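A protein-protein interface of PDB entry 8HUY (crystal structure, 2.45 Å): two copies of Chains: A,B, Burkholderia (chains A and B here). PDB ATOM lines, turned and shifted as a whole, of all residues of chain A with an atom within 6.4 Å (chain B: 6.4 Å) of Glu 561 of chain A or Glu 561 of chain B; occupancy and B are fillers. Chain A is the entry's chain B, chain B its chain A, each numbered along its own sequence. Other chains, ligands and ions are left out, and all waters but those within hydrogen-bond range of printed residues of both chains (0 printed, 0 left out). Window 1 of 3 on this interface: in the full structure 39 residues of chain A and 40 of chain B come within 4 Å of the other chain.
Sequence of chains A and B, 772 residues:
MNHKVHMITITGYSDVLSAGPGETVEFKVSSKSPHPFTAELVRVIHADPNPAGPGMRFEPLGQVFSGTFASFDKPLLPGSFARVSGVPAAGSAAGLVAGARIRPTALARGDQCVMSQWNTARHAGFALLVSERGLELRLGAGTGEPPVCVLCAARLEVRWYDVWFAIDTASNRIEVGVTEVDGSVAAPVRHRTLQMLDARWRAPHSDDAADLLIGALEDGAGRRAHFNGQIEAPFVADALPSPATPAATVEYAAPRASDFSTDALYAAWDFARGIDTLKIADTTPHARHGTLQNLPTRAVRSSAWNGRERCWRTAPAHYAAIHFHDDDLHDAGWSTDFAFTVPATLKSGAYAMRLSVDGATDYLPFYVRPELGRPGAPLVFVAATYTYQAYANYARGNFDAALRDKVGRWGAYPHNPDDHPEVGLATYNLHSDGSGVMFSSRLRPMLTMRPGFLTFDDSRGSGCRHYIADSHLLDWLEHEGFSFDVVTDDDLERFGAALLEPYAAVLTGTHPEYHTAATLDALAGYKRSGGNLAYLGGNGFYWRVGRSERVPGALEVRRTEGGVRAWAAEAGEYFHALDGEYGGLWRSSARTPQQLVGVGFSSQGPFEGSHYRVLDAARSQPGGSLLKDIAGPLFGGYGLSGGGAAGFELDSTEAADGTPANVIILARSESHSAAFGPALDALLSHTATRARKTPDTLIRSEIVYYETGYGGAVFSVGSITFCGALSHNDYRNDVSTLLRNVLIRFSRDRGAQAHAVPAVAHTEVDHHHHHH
Printed residues of chain B that touch a printed residue of chain A: Arg 310, Glu 561, Arg 565, Ala 571, Tyr 574, Tyr 582, Ser 588, Ser 589 and Arg 690. Of the 17 printed residues of chain A, 9 touch a printed residue of chain B. Hydrophobic or aromatic side chains of chain A within 4 Å of the printed part of chain B: Ala 571, Tyr 574 and Tyr 582. Among the printed residues, 15 pairs touch across the chains. Among the printed residues, no Asp or Glu carboxylate lies within 4 Å of a Lys or Arg side-chain nitrogen of the other chain.
The backbone carbonyl oxygen of Ser 588 of chain B is in hydrogen-bond range of the guanidinium group of Arg 310 of chain A (3.0 Å). The guanidinium group of Arg 310 of chain B lies within hydrogen-bond range of the backbone carbonyl oxygen of Ser 588 of chain A. The guanidinium group (NH2) of Arg 310 of chain B is in hydrogen-bond range of the side-chain hydroxyl (OG) of Ser 589 of chain A, at 2.9 Å. The side-chain carboxylate (OE1) of Glu 561 of chain B sits at hydrogen-bond distance from the side-chain hydroxyl (OH) of Tyr 574 of chain A (2.6 Å). OG of Ser 589 of chain B lies within hydrogen-bond range of NH2 of Arg 310 of chain A, 3.2 Å away. The side-chain carboxylate (OE1) of Glu 561 of chain A lies within hydrogen-bond range of the side-chain hydroxyl (OH) of Tyr 574 of chain B (2.6 Å).
Of chain A, only Glu 561 (3.4 Å) and Tyr 574 (2.6 Å) come within 4 Å of Glu 561 of chain B. Printed residues of chain A within 4 Å of Arg 565 of chain B: Arg 690 (3.98 Å). Of the printed residues of chain A, Ser 588 of chain B touches Arg 310 and Ala 571. Gly 584 of chain A touches none of the printed residues of chain B. Gly 563 of chain A touches none of the printed residues of chain B. The nearest residue of chain B that does not touch Glu 561 of chain A is Gly 562 of chain B (4.6 Å). The nearest residue of chain A that does not touch Glu 561 of chain B is Gly 562 of chain A (4.7 Å).
NH1 of Arg 565 of chain B lies within hydrogen-bond range of O of Glu 561 of chain B (3.4 Å). The side-chain carboxylate of Glu 561 of chain B is in hydrogen-bond range of the side-chain hydroxyl of Tyr 582 of chain B (2.4 Å). The backbone carbonyl oxygen (O) of Gly 562 of chain B sits close to the guanidinium group (NE) of Arg 565 of chain B (3.4 Å). The side-chain carboxylate of Glu 561 of chain A sits close to the side-chain hydroxyl of Ser 588 of chain A (3.1 Å). The backbone carbonyl oxygen (O) of Arg 559 of chain B sits at hydrogen-bond distance from the guanidinium group (NH2) of Arg 565 of chain B, at 2.7 Å. OH of Tyr 582 of chain A sits at hydrogen-bond distance from OE2 of Glu 561 of chain A.
CD1 of Tyr 582 of chain B touches NH1 of Arg 310 of chain A (3.3 Å). Glu 561 of chain B touches Glu 561 of chain A. NH1 of Arg 565 of chain A touches NH2 of Arg 690 of chain B, 3.98 Å away. O of Ser 588 of chain B touches CB of Ala 571 of chain A, at 3.4 Å. Tyr 574 of chain A touches Tyr 582 of chain B (CE2 to OH, 3.9 Å). Arg 310 of chain B touches Tyr 582 of chain A. Tyr 574 of chain B touches Tyr 582 of chain A (CE2 to OH, 3.9 Å). Ala 571 of chain B touches Ser 588 of chain A. NH1 of Arg 565 of chain B touches NH2 of Arg 690 of chain A, 3.98 Å away.
Arg 310 of chain A touches Ser 588 of chain B, and with the chains exchanged Ser 588 of chain A touches Arg 310 of chain B. Glu 561 of chain B touches its own counterpart, Glu 561 of chain A. Arg 565 of chain A touches Arg 690 of chain B, and with the chains exchanged Arg 690 of chain A touches Arg 565 of chain B. Tyr 574 of chain A touches Tyr 582 of chain B, and with the chains exchanged Tyr 582 of chain A touches Tyr 574 of chain B. 17 positions are printed for both chains. Of the 15 pairs that touch across the chains among the printed residues, 15 have their exchanged pair printed and touching as well.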
ATOM      1  N   ARG A 310     -20.258  15.769 -30.148  1.00  0.00           N
ATOM      2  CA  ARG A 310     -19.559  16.103 -28.915  1.00  0.00           C
ATOM      3  C   ARG A 310     -20.471  16.734 -27.872  1.00  0.00           C
ATOM      4  O   ARG A 310     -19.983  17.149 -26.814  1.00  0.00           O
ATOM      5  CB  ARG A 310     -18.400  17.069 -29.197  1.00  0.00           C
ATOM      6  CG  ARG A 310     -17.470  16.619 -30.307  1.00  0.00           C
ATOM      7  CD  ARG A 310     -16.825  15.278 -29.963  1.00  0.00           C
ATOM      8  NE  ARG A 310     -16.116  14.701 -31.103  1.00  0.00           N
ATOM      9  CZ  ARG A 310     -14.794  14.632 -31.198  1.00  0.00           C
ATOM     10  NH1 ARG A 310     -14.041  15.124 -30.223  1.00  0.00           N
ATOM     11  NH2 ARG A 310     -14.229  14.078 -32.268  1.00  0.00           N
ATOM     12  N   ARG A 559     -12.730  18.364 -16.157  1.00  0.00           N
ATOM     13  CA  ARG A 559     -11.465  19.060 -16.370  1.00  0.00           C
ATOM     14  C   ARG A 559     -11.071  18.884 -17.835  1.00  0.00           C
ATOM     15  O   ARG A 559     -10.354  17.950 -18.207  1.00  0.00           O
ATOM     16  CB  ARG A 559     -10.435  18.546 -15.374  1.00  0.00           C
ATOM     17  CG  ARG A 559     -11.019  18.376 -13.946  1.00  0.00           C
ATOM     18  CD  ARG A 559      -9.902  18.254 -12.905  1.00  0.00           C
ATOM     19  NE  ARG A 559     -10.331  18.314 -11.507  1.00  0.00           N
ATOM     20  CZ  ARG A 559     -10.502  19.432 -10.788  1.00  0.00           C
ATOM     21  NH1 ARG A 559     -10.315  20.633 -11.317  1.00  0.00           N
ATOM     22  NH2 ARG A 559     -10.860  19.354  -9.515  1.00  0.00           N
ATOM     23  N   THR A 560     -11.571  19.794 -18.683  1.00  0.00           N
ATOM     24  CA  THR A 560     -11.476  19.661 -20.134  1.00  0.00           C
ATOM     25  C   THR A 560     -10.261  20.390 -20.714  1.00  0.00           C
ATOM     26  O   THR A 560      -9.702  21.312 -20.110  1.00  0.00           O
ATOM     27  CB  THR A 560     -12.765  20.161 -20.797  1.00  0.00           C
ATOM     28  OG1 THR A 560     -12.840  21.600 -20.760  1.00  0.00           O
ATOM     29  CG2 THR A 560     -13.968  19.561 -20.064  1.00  0.00           C
ATOM     30  N   GLU A 561      -9.862  19.949 -21.915  1.00  0.00           N
ATOM     31  CA  GLU A 561      -8.876  20.612 -22.776  1.00  0.00           C
ATOM     32  C   GLU A 561      -7.440  20.533 -22.256  1.00  0.00           C
ATOM     33  O   GLU A 561      -6.589  19.924 -22.901  1.00  0.00           O
ATOM     34  CB  GLU A 561      -9.263  22.072 -23.020  1.00  0.00           C
ATOM     35  CG  GLU A 561     -10.607  22.205 -23.692  1.00  0.00           C
ATOM     36  CD  GLU A 561     -10.770  23.465 -24.534  1.00  0.00           C
ATOM     37  OE1 GLU A 561      -9.741  24.054 -24.969  1.00  0.00           O
ATOM     38  OE2 GLU A 561     -11.943  23.827 -24.804  1.00  0.00           O
ATOM     39  N   GLY A 562      -7.141  21.182 -21.134  1.00  0.00           N
ATOM     40  CA  GLY A 562      -5.787  21.235 -20.606  1.00  0.00           C
ATOM     41  C   GLY A 562      -5.753  21.967 -19.279  1.00  0.00           C
ATOM     42  O   GLY A 562      -6.672  21.830 -18.472  1.00  0.00           O
ATOM     43  N   GLY A 563      -4.715  22.760 -19.041  1.00  0.00           N
ATOM     44  CA  GLY A 563      -4.583  23.451 -17.776  1.00  0.00           C
ATOM     45  C   GLY A 563      -3.939  22.552 -16.743  1.00  0.00           C
ATOM     46  O   GLY A 563      -3.614  21.388 -16.998  1.00  0.00           O
ATOM     47  N   ARG A 565      -4.389  20.274 -13.963  1.00  0.00           N
ATOM     48  CA  ARG A 565      -5.605  19.498 -13.731  1.00  0.00           C
ATOM     49  C   ARG A 565      -5.229  18.168 -13.098  1.00  0.00           C
ATOM     50  O   ARG A 565      -4.273  17.516 -13.529  1.00  0.00           O
ATOM     51  CB  ARG A 565      -6.403  19.270 -15.058  1.00  0.00           C
ATOM     52  CG  ARG A 565      -5.664  18.428 -16.135  1.00  0.00           C
ATOM     53  CD  ARG A 565      -5.783  18.928 -17.588  1.00  0.00           C
ATOM     54  NE  ARG A 565      -7.028  18.534 -18.231  1.00  0.00           N
ATOM     55  CZ  ARG A 565      -7.158  18.062 -19.477  1.00  0.00           C
ATOM     56  NH1 ARG A 565      -6.097  17.876 -20.276  1.00  0.00           N
ATOM     57  NH2 ARG A 565      -8.381  17.751 -19.924  1.00  0.00           N
ATOM     58  N   ALA A 569     -10.572  15.025 -18.623  1.00  0.00           N
ATOM     59  CA  ALA A 569     -11.824  14.545 -19.187  1.00  0.00           C
ATOM     60  C   ALA A 569     -11.582  13.830 -20.508  1.00  0.00           C
ATOM     61  O   ALA A 569     -10.667  14.178 -21.266  1.00  0.00           O
ATOM     62  CB  ALA A 569     -12.778  15.716 -19.421  1.00  0.00           C
ATOM     63  N   ALA A 571     -12.424  12.939 -24.380  1.00  0.00           N
ATOM     64  CA  ALA A 571     -12.974  13.607 -25.552  1.00  0.00           C
ATOM     65  C   ALA A 571     -14.459  13.309 -25.684  1.00  0.00           C
ATOM     66  O   ALA A 571     -14.896  12.162 -25.517  1.00  0.00           O
ATOM     67  CB  ALA A 571     -12.240  13.134 -26.800  1.00  0.00           C
ATOM     68  N   TYR A 574     -17.339  16.745 -22.581  1.00  0.00           N
ATOM     69  CA  TYR A 574     -16.961  18.060 -22.093  1.00  0.00           C
ATOM     70  C   TYR A 574     -18.131  18.863 -21.534  1.00  0.00           C
ATOM     71  O   TYR A 574     -17.892  19.866 -20.849  1.00  0.00           O
ATOM     72  CB  TYR A 574     -16.302  18.858 -23.223  1.00  0.00           C
ATOM     73  CG  TYR A 574     -14.875  18.468 -23.518  1.00  0.00           C
ATOM     74  CD1 TYR A 574     -14.271  17.386 -22.870  1.00  0.00           C
ATOM     75  CD2 TYR A 574     -14.123  19.183 -24.457  1.00  0.00           C
ATOM     76  CE1 TYR A 574     -12.952  17.028 -23.151  1.00  0.00           C
ATOM     77  CE2 TYR A 574     -12.809  18.829 -24.746  1.00  0.00           C
ATOM     78  CZ  TYR A 574     -12.218  17.752 -24.087  1.00  0.00           C
ATOM     79  OH  TYR A 574     -10.908  17.416 -24.373  1.00  0.00           O
ATOM     80  N   TYR A 582     -20.746  23.925 -21.209  1.00  0.00           N
ATOM     81  CA  TYR A 582     -19.397  23.507 -21.579  1.00  0.00           C
ATOM     82  C   TYR A 582     -18.482  23.704 -20.388  1.00  0.00           C
ATOM     83  O   TYR A 582     -18.328  24.821 -19.905  1.00  0.00           O
ATOM     84  CB  TYR A 582     -18.886  24.328 -22.775  1.00  0.00           C
ATOM     85  CG  TYR A 582     -17.586  23.834 -23.419  1.00  0.00           C
ATOM     86  CD1 TYR A 582     -16.340  24.323 -23.018  1.00  0.00           C
ATOM     87  CD2 TYR A 582     -17.609  22.894 -24.434  1.00  0.00           C
ATOM     88  CE1 TYR A 582     -15.142  23.869 -23.616  1.00  0.00           C
ATOM     89  CE2 TYR A 582     -16.437  22.423 -25.022  1.00  0.00           C
ATOM     90  CZ  TYR A 582     -15.215  22.906 -24.610  1.00  0.00           C
ATOM     91  OH  TYR A 582     -14.096  22.441 -25.229  1.00  0.00           O
ATOM     92  N   GLY A 583     -17.884  22.628 -19.904  1.00  0.00           N
ATOM     93  CA  GLY A 583     -17.097  22.673 -18.692  1.00  0.00           C
ATOM     94  C   GLY A 583     -15.634  22.963 -18.966  1.00  0.00           C
ATOM     95  O   GLY A 583     -15.219  23.260 -20.090  1.00  0.00           O
ATOM     96  N   GLY A 584     -14.851  22.886 -17.892  1.00  0.00           N
ATOM     97  CA  GLY A 584     -13.424  23.056 -17.942  1.00  0.00           C
ATOM     98  C   GLY A 584     -12.983  24.433 -17.492  1.00  0.00           C
ATOM     99  O   GLY A 584     -13.621  25.062 -16.636  1.00  0.00           O
ATOM    100  N   LEU A 585     -11.876  24.900 -18.073  1.00  0.00           N
ATOM    101  CA  LEU A 585     -11.315  26.189 -17.709  1.00  0.00           C
ATOM    102  C   LEU A 585     -12.179  27.313 -18.249  1.00  0.00           C
ATOM    103  O   LEU A 585     -12.731  27.220 -19.350  1.00  0.00           O
ATOM    104  CB  LEU A 585      -9.892  26.319 -18.238  1.00  0.00           C
ATOM    105  CG  LEU A 585      -8.998  25.303 -17.529  1.00  0.00           C
ATOM    106  CD1 LEU A 585      -8.580  24.229 -18.527  1.00  0.00           C
ATOM    107  CD2 LEU A 585      -7.800  25.966 -16.885  1.00  0.00           C
ATOM    108  N   SER A 588     -11.384  28.424 -21.572  1.00  0.00           N
ATOM    109  CA  SER A 588     -12.069  27.683 -22.634  1.00  0.00           C
ATOM    110  C   SER A 588     -13.516  28.072 -22.783  1.00  0.00           C
ATOM    111  O   SER A 588     -14.205  27.518 -23.645  1.00  0.00           O
ATOM    112  CB  SER A 588     -11.970  26.178 -22.399  1.00  0.00           C
ATOM    113  OG  SER A 588     -10.633  25.748 -22.533  1.00  0.00           O
ATOM    114  N   SER A 589     -13.990  29.014 -21.990  1.00  0.00           N
ATOM    115  CA  SER A 589     -15.278  29.649 -22.235  1.00  0.00           C
ATOM    116  C   SER A 589     -15.094  31.156 -22.327  1.00  0.00           C
ATOM    117  O   SER A 589     -15.956  31.942 -21.915  1.00  0.00           O
ATOM    118  CB  SER A 589     -16.273  29.290 -21.123  1.00  0.00           C
ATOM    119  OG  SER A 589     -16.733  27.961 -21.284  1.00  0.00           O
ATOM    120  N   ARG A 690       1.657  31.814 -24.599  1.00  0.00           N
ATOM    121  CA  ARG A 690       0.743  32.302 -25.623  1.00  0.00           C
ATOM    122  C   ARG A 690       1.167  33.671 -26.136  1.00  0.00           C
ATOM    123  O   ARG A 690       1.003  33.968 -27.327  1.00  0.00           O
ATOM    124  CB  ARG A 690      -0.683  32.369 -25.078  1.00  0.00           C
ATOM    125  CG  ARG A 690      -1.351  31.027 -24.822  1.00  0.00           C
ATOM    126  CD  ARG A 690      -2.712  31.248 -24.182  1.00  0.00           C
ATOM    127  NE  ARG A 690      -3.430  30.000 -24.002  1.00  0.00           N
ATOM    128  CZ  ARG A 690      -4.373  29.578 -24.835  1.00  0.00           C
ATOM    129  NH1 ARG A 690      -4.703  30.328 -25.883  1.00  0.00           N
ATOM    130  NH2 ARG A 690      -4.991  28.417 -24.617  1.00  0.00           N
ATOM    131  N   ARG B 310     -21.272  25.732 -29.289  1.00  0.00           N
ATOM    132  CA  ARG B 310     -19.893  25.517 -29.718  1.00  0.00           C
ATOM    133  C   ARG B 310     -19.788  24.840 -31.078  1.00  0.00           C
ATOM    134  O   ARG B 310     -18.667  24.532 -31.508  1.00  0.00           O
ATOM    135  CB  ARG B 310     -19.107  24.633 -28.709  1.00  0.00           C
ATOM    136  CG  ARG B 310     -19.156  25.058 -27.261  1.00  0.00           C
ATOM    137  CD  ARG B 310     -18.401  26.362 -27.022  1.00  0.00           C
ATOM    138  NE  ARG B 310     -18.794  27.013 -25.763  1.00  0.00           N
ATOM    139  CZ  ARG B 310     -17.962  27.308 -24.763  1.00  0.00           C
ATOM    140  NH1 ARG B 310     -16.667  27.011 -24.854  1.00  0.00           N
ATOM    141  NH2 ARG B 310     -18.435  27.900 -23.660  1.00  0.00           N
ATOM    142  N   ARG B 559      -6.010  24.352 -34.310  1.00  0.00           N
ATOM    143  CA  ARG B 559      -5.165  23.835 -33.245  1.00  0.00           C
ATOM    144  C   ARG B 559      -5.928  23.977 -31.930  1.00  0.00           C
ATOM    145  O   ARG B 559      -5.765  24.946 -31.184  1.00  0.00           O
ATOM    146  CB  ARG B 559      -3.824  24.563 -33.267  1.00  0.00           C
ATOM    147  CG  ARG B 559      -3.280  24.653 -34.687  1.00  0.00           C
ATOM    148  CD  ARG B 559      -1.789  24.943 -34.761  1.00  0.00           C
ATOM    149  NE  ARG B 559      -1.261  24.763 -36.112  1.00  0.00           N
ATOM    150  CZ  ARG B 559      -0.694  23.638 -36.551  1.00  0.00           C
ATOM    151  NH1 ARG B 559      -0.587  22.585 -35.746  1.00  0.00           N
ATOM    152  NH2 ARG B 559      -0.228  23.566 -37.800  1.00  0.00           N
ATOM    153  N   THR B 560      -6.748  22.972 -31.623  1.00  0.00           N
ATOM    154  CA  THR B 560      -7.661  23.086 -30.504  1.00  0.00           C
ATOM    155  C   THR B 560      -7.017  22.562 -29.225  1.00  0.00           C
ATOM    156  O   THR B 560      -6.005  21.858 -29.252  1.00  0.00           O
ATOM    157  CB  THR B 560      -8.970  22.330 -30.783  1.00  0.00           C
ATOM    158  OG1 THR B 560      -8.721  20.917 -30.885  1.00  0.00           O
ATOM    159  CG2 THR B 560      -9.614  22.825 -32.055  1.00  0.00           C
ATOM    160  N   GLU B 561      -7.584  23.003 -28.095  1.00  0.00           N
ATOM    161  CA  GLU B 561      -7.384  22.454 -26.752  1.00  0.00           C
ATOM    162  C   GLU B 561      -6.020  22.702 -26.125  1.00  0.00           C
ATOM    163  O   GLU B 561      -5.933  23.416 -25.121  1.00  0.00           O
ATOM    164  CB  GLU B 561      -7.675  20.944 -26.750  1.00  0.00           C
ATOM    165  CG  GLU B 561      -9.136  20.691 -27.023  1.00  0.00           C
ATOM    166  CD  GLU B 561      -9.623  19.340 -26.600  1.00  0.00           C
ATOM    167  OE1 GLU B 561      -9.127  18.774 -25.593  1.00  0.00           O
ATOM    168  OE2 GLU B 561     -10.516  18.844 -27.304  1.00  0.00           O
ATOM    169  N   GLY B 562      -4.971  22.090 -26.677  1.00  0.00           N
ATOM    170  CA  GLY B 562      -3.627  22.164 -26.136  1.00  0.00           C
ATOM    171  C   GLY B 562      -2.649  21.499 -27.081  1.00  0.00           C
ATOM    172  O   GLY B 562      -2.866  21.542 -28.298  1.00  0.00           O
ATOM    173  N   GLY B 563      -1.604  20.843 -26.547  1.00  0.00           N
ATOM    174  CA  GLY B 563      -0.569  20.251 -27.372  1.00  0.00           C
ATOM    175  C   GLY B 563       0.515  21.257 -27.748  1.00  0.00           C
ATOM    176  O   GLY B 563       0.482  22.440 -27.383  1.00  0.00           O
ATOM    177  N   ARG B 565       1.857  23.586 -30.234  1.00  0.00           N
ATOM    178  CA  ARG B 565       1.080  24.265 -31.269  1.00  0.00           C
ATOM    179  C   ARG B 565       1.642  25.653 -31.546  1.00  0.00           C
ATOM    180  O   ARG B 565       2.039  26.367 -30.622  1.00  0.00           O
ATOM    181  CB  ARG B 565      -0.402  24.383 -30.862  1.00  0.00           C
ATOM    182  CG  ARG B 565      -0.612  25.169 -29.566  1.00  0.00           C
ATOM    183  CD  ARG B 565      -1.659  24.557 -28.631  1.00  0.00           C
ATOM    184  NE  ARG B 565      -3.035  24.861 -29.012  1.00  0.00           N
ATOM    185  CZ  ARG B 565      -3.989  25.242 -28.157  1.00  0.00           C
ATOM    186  NH1 ARG B 565      -3.721  25.391 -26.861  1.00  0.00           N
ATOM    187  NH2 ARG B 565      -5.221  25.464 -28.595  1.00  0.00           N
ATOM    188  N   ALA B 569      -6.441  27.817 -31.218  1.00  0.00           N
ATOM    189  CA  ALA B 569      -7.793  28.161 -31.640  1.00  0.00           C
ATOM    190  C   ALA B 569      -8.549  28.838 -30.499  1.00  0.00           C
ATOM    191  O   ALA B 569      -8.315  28.558 -29.315  1.00  0.00           O
ATOM    192  CB  ALA B 569      -8.544  26.913 -32.102  1.00  0.00           C
ATOM    193  N   ALA B 571     -11.934  29.603 -28.293  1.00  0.00           N
ATOM    194  CA  ALA B 571     -13.081  28.855 -27.803  1.00  0.00           C
ATOM    195  C   ALA B 571     -14.271  28.975 -28.747  1.00  0.00           C
ATOM    196  O   ALA B 571     -14.607  30.072 -29.219  1.00  0.00           O
ATOM    197  CB  ALA B 571     -13.454  29.363 -26.414  1.00  0.00           C
ATOM    198  N   TYR B 574     -13.796  25.343 -32.794  1.00  0.00           N
ATOM    199  CA  TYR B 574     -13.046  24.101 -32.800  1.00  0.00           C
ATOM    200  C   TYR B 574     -13.429  23.195 -33.960  1.00  0.00           C
ATOM    201  O   TYR B 574     -12.673  22.272 -34.294  1.00  0.00           O
ATOM    202  CB  TYR B 574     -13.268  23.366 -31.462  1.00  0.00           C
ATOM    203  CG  TYR B 574     -12.436  23.906 -30.306  1.00  0.00           C
ATOM    204  CD1 TYR B 574     -11.618  25.027 -30.474  1.00  0.00           C
ATOM    205  CD2 TYR B 574     -12.450  23.288 -29.049  1.00  0.00           C
ATOM    206  CE1 TYR B 574     -10.824  25.517 -29.425  1.00  0.00           C
ATOM    207  CE2 TYR B 574     -11.667  23.771 -28.000  1.00  0.00           C
ATOM    208  CZ  TYR B 574     -10.848  24.897 -28.197  1.00  0.00           C
ATOM    209  OH  TYR B 574     -10.056  25.396 -27.178  1.00  0.00           O
ATOM    210  N   TYR B 582     -14.703  17.886 -35.762  1.00  0.00           N
ATOM    211  CA  TYR B 582     -13.987  18.443 -34.617  1.00  0.00           C
ATOM    212  C   TYR B 582     -12.480  18.350 -34.843  1.00  0.00           C
ATOM    213  O   TYR B 582     -11.931  17.252 -34.951  1.00  0.00           O
ATOM    214  CB  TYR B 582     -14.389  17.682 -33.351  1.00  0.00           C
ATOM    215  CG  TYR B 582     -13.825  18.243 -32.068  1.00  0.00           C
ATOM    216  CD1 TYR B 582     -12.623  17.771 -31.542  1.00  0.00           C
ATOM    217  CD2 TYR B 582     -14.518  19.218 -31.360  1.00  0.00           C
ATOM    218  CE1 TYR B 582     -12.110  18.288 -30.344  1.00  0.00           C
ATOM    219  CE2 TYR B 582     -14.024  19.738 -30.171  1.00  0.00           C
ATOM    220  CZ  TYR B 582     -12.822  19.281 -29.679  1.00  0.00           C
ATOM    221  OH  TYR B 582     -12.362  19.819 -28.526  1.00  0.00           O
ATOM    222  N   GLY B 583     -11.801  19.493 -34.895  1.00  0.00           N
ATOM    223  CA  GLY B 583     -10.399  19.537 -35.254  1.00  0.00           C
ATOM    224  C   GLY B 583      -9.481  19.471 -34.053  1.00  0.00           C
ATOM    225  O   GLY B 583      -9.902  19.303 -32.907  1.00  0.00           O
ATOM    226  N   GLY B 584      -8.194  19.628 -34.332  1.00  0.00           N
ATOM    227  CA  GLY B 584      -7.196  19.627 -33.288  1.00  0.00           C
ATOM    228  C   GLY B 584      -6.429  18.330 -33.198  1.00  0.00           C
ATOM    229  O   GLY B 584      -6.241  17.635 -34.201  1.00  0.00           O
ATOM    230  N   LEU B 585      -5.983  17.996 -31.992  1.00  0.00           N
ATOM    231  CA  LEU B 585      -5.188  16.799 -31.799  1.00  0.00           C
ATOM    232  C   LEU B 585      -6.052  15.560 -31.984  1.00  0.00           C
ATOM    233  O   LEU B 585      -7.210  15.530 -31.551  1.00  0.00           O
ATOM    234  CB  LEU B 585      -4.598  16.797 -30.399  1.00  0.00           C
ATOM    235  CG  LEU B 585      -3.783  17.971 -29.899  1.00  0.00           C
ATOM    236  CD1 LEU B 585      -3.578  17.723 -28.422  1.00  0.00           C
ATOM    237  CD2 LEU B 585      -2.435  18.059 -30.596  1.00  0.00           C
ATOM    238  N   SER B 588      -7.601  14.458 -28.963  1.00  0.00           N
ATOM    239  CA  SER B 588      -8.898  15.074 -28.710  1.00  0.00           C
ATOM    240  C   SER B 588     -10.017  14.537 -29.605  1.00  0.00           C
ATOM    241  O   SER B 588     -11.157  14.988 -29.441  1.00  0.00           O
ATOM    242  CB  SER B 588      -8.795  16.594 -28.815  1.00  0.00           C
ATOM    243  OG  SER B 588      -7.736  17.082 -27.998  1.00  0.00           O
ATOM    244  N   SER B 589      -9.755  13.583 -30.502  1.00  0.00           N
ATOM    245  CA  SER B 589     -10.833  12.813 -31.108  1.00  0.00           C
ATOM    246  C   SER B 589     -10.624  11.330 -30.854  1.00  0.00           C
ATOM    247  O   SER B 589     -10.970  10.480 -31.672  1.00  0.00           O
ATOM    248  CB  SER B 589     -10.967  13.085 -32.610  1.00  0.00           C
ATOM    249  OG  SER B 589     -11.151  14.440 -32.900  1.00  0.00           O
ATOM    250  N   ARG B 690       0.224  12.294 -17.820  1.00  0.00           N
ATOM    251  CA  ARG B 690      -1.097  11.685 -17.692  1.00  0.00           C
ATOM    252  C   ARG B 690      -1.044  10.367 -16.927  1.00  0.00           C
ATOM    253  O   ARG B 690      -2.010  10.020 -16.235  1.00  0.00           O
ATOM    254  CB  ARG B 690      -1.725  11.461 -19.067  1.00  0.00           C
ATOM    255  CG  ARG B 690      -2.430  12.670 -19.650  1.00  0.00           C
ATOM    256  CD  ARG B 690      -2.720  12.434 -21.108  1.00  0.00           C
ATOM    257  NE  ARG B 690      -3.320  13.588 -21.772  1.00  0.00           N
ATOM    258  CZ  ARG B 690      -4.629  13.714 -21.950  1.00  0.00           C
ATOM    259  NH1 ARG B 690      -5.427  12.746 -21.508  1.00  0.00           N
ATOM    260  NH2 ARG B 690      -5.132  14.772 -22.579  1.00  0.00           N
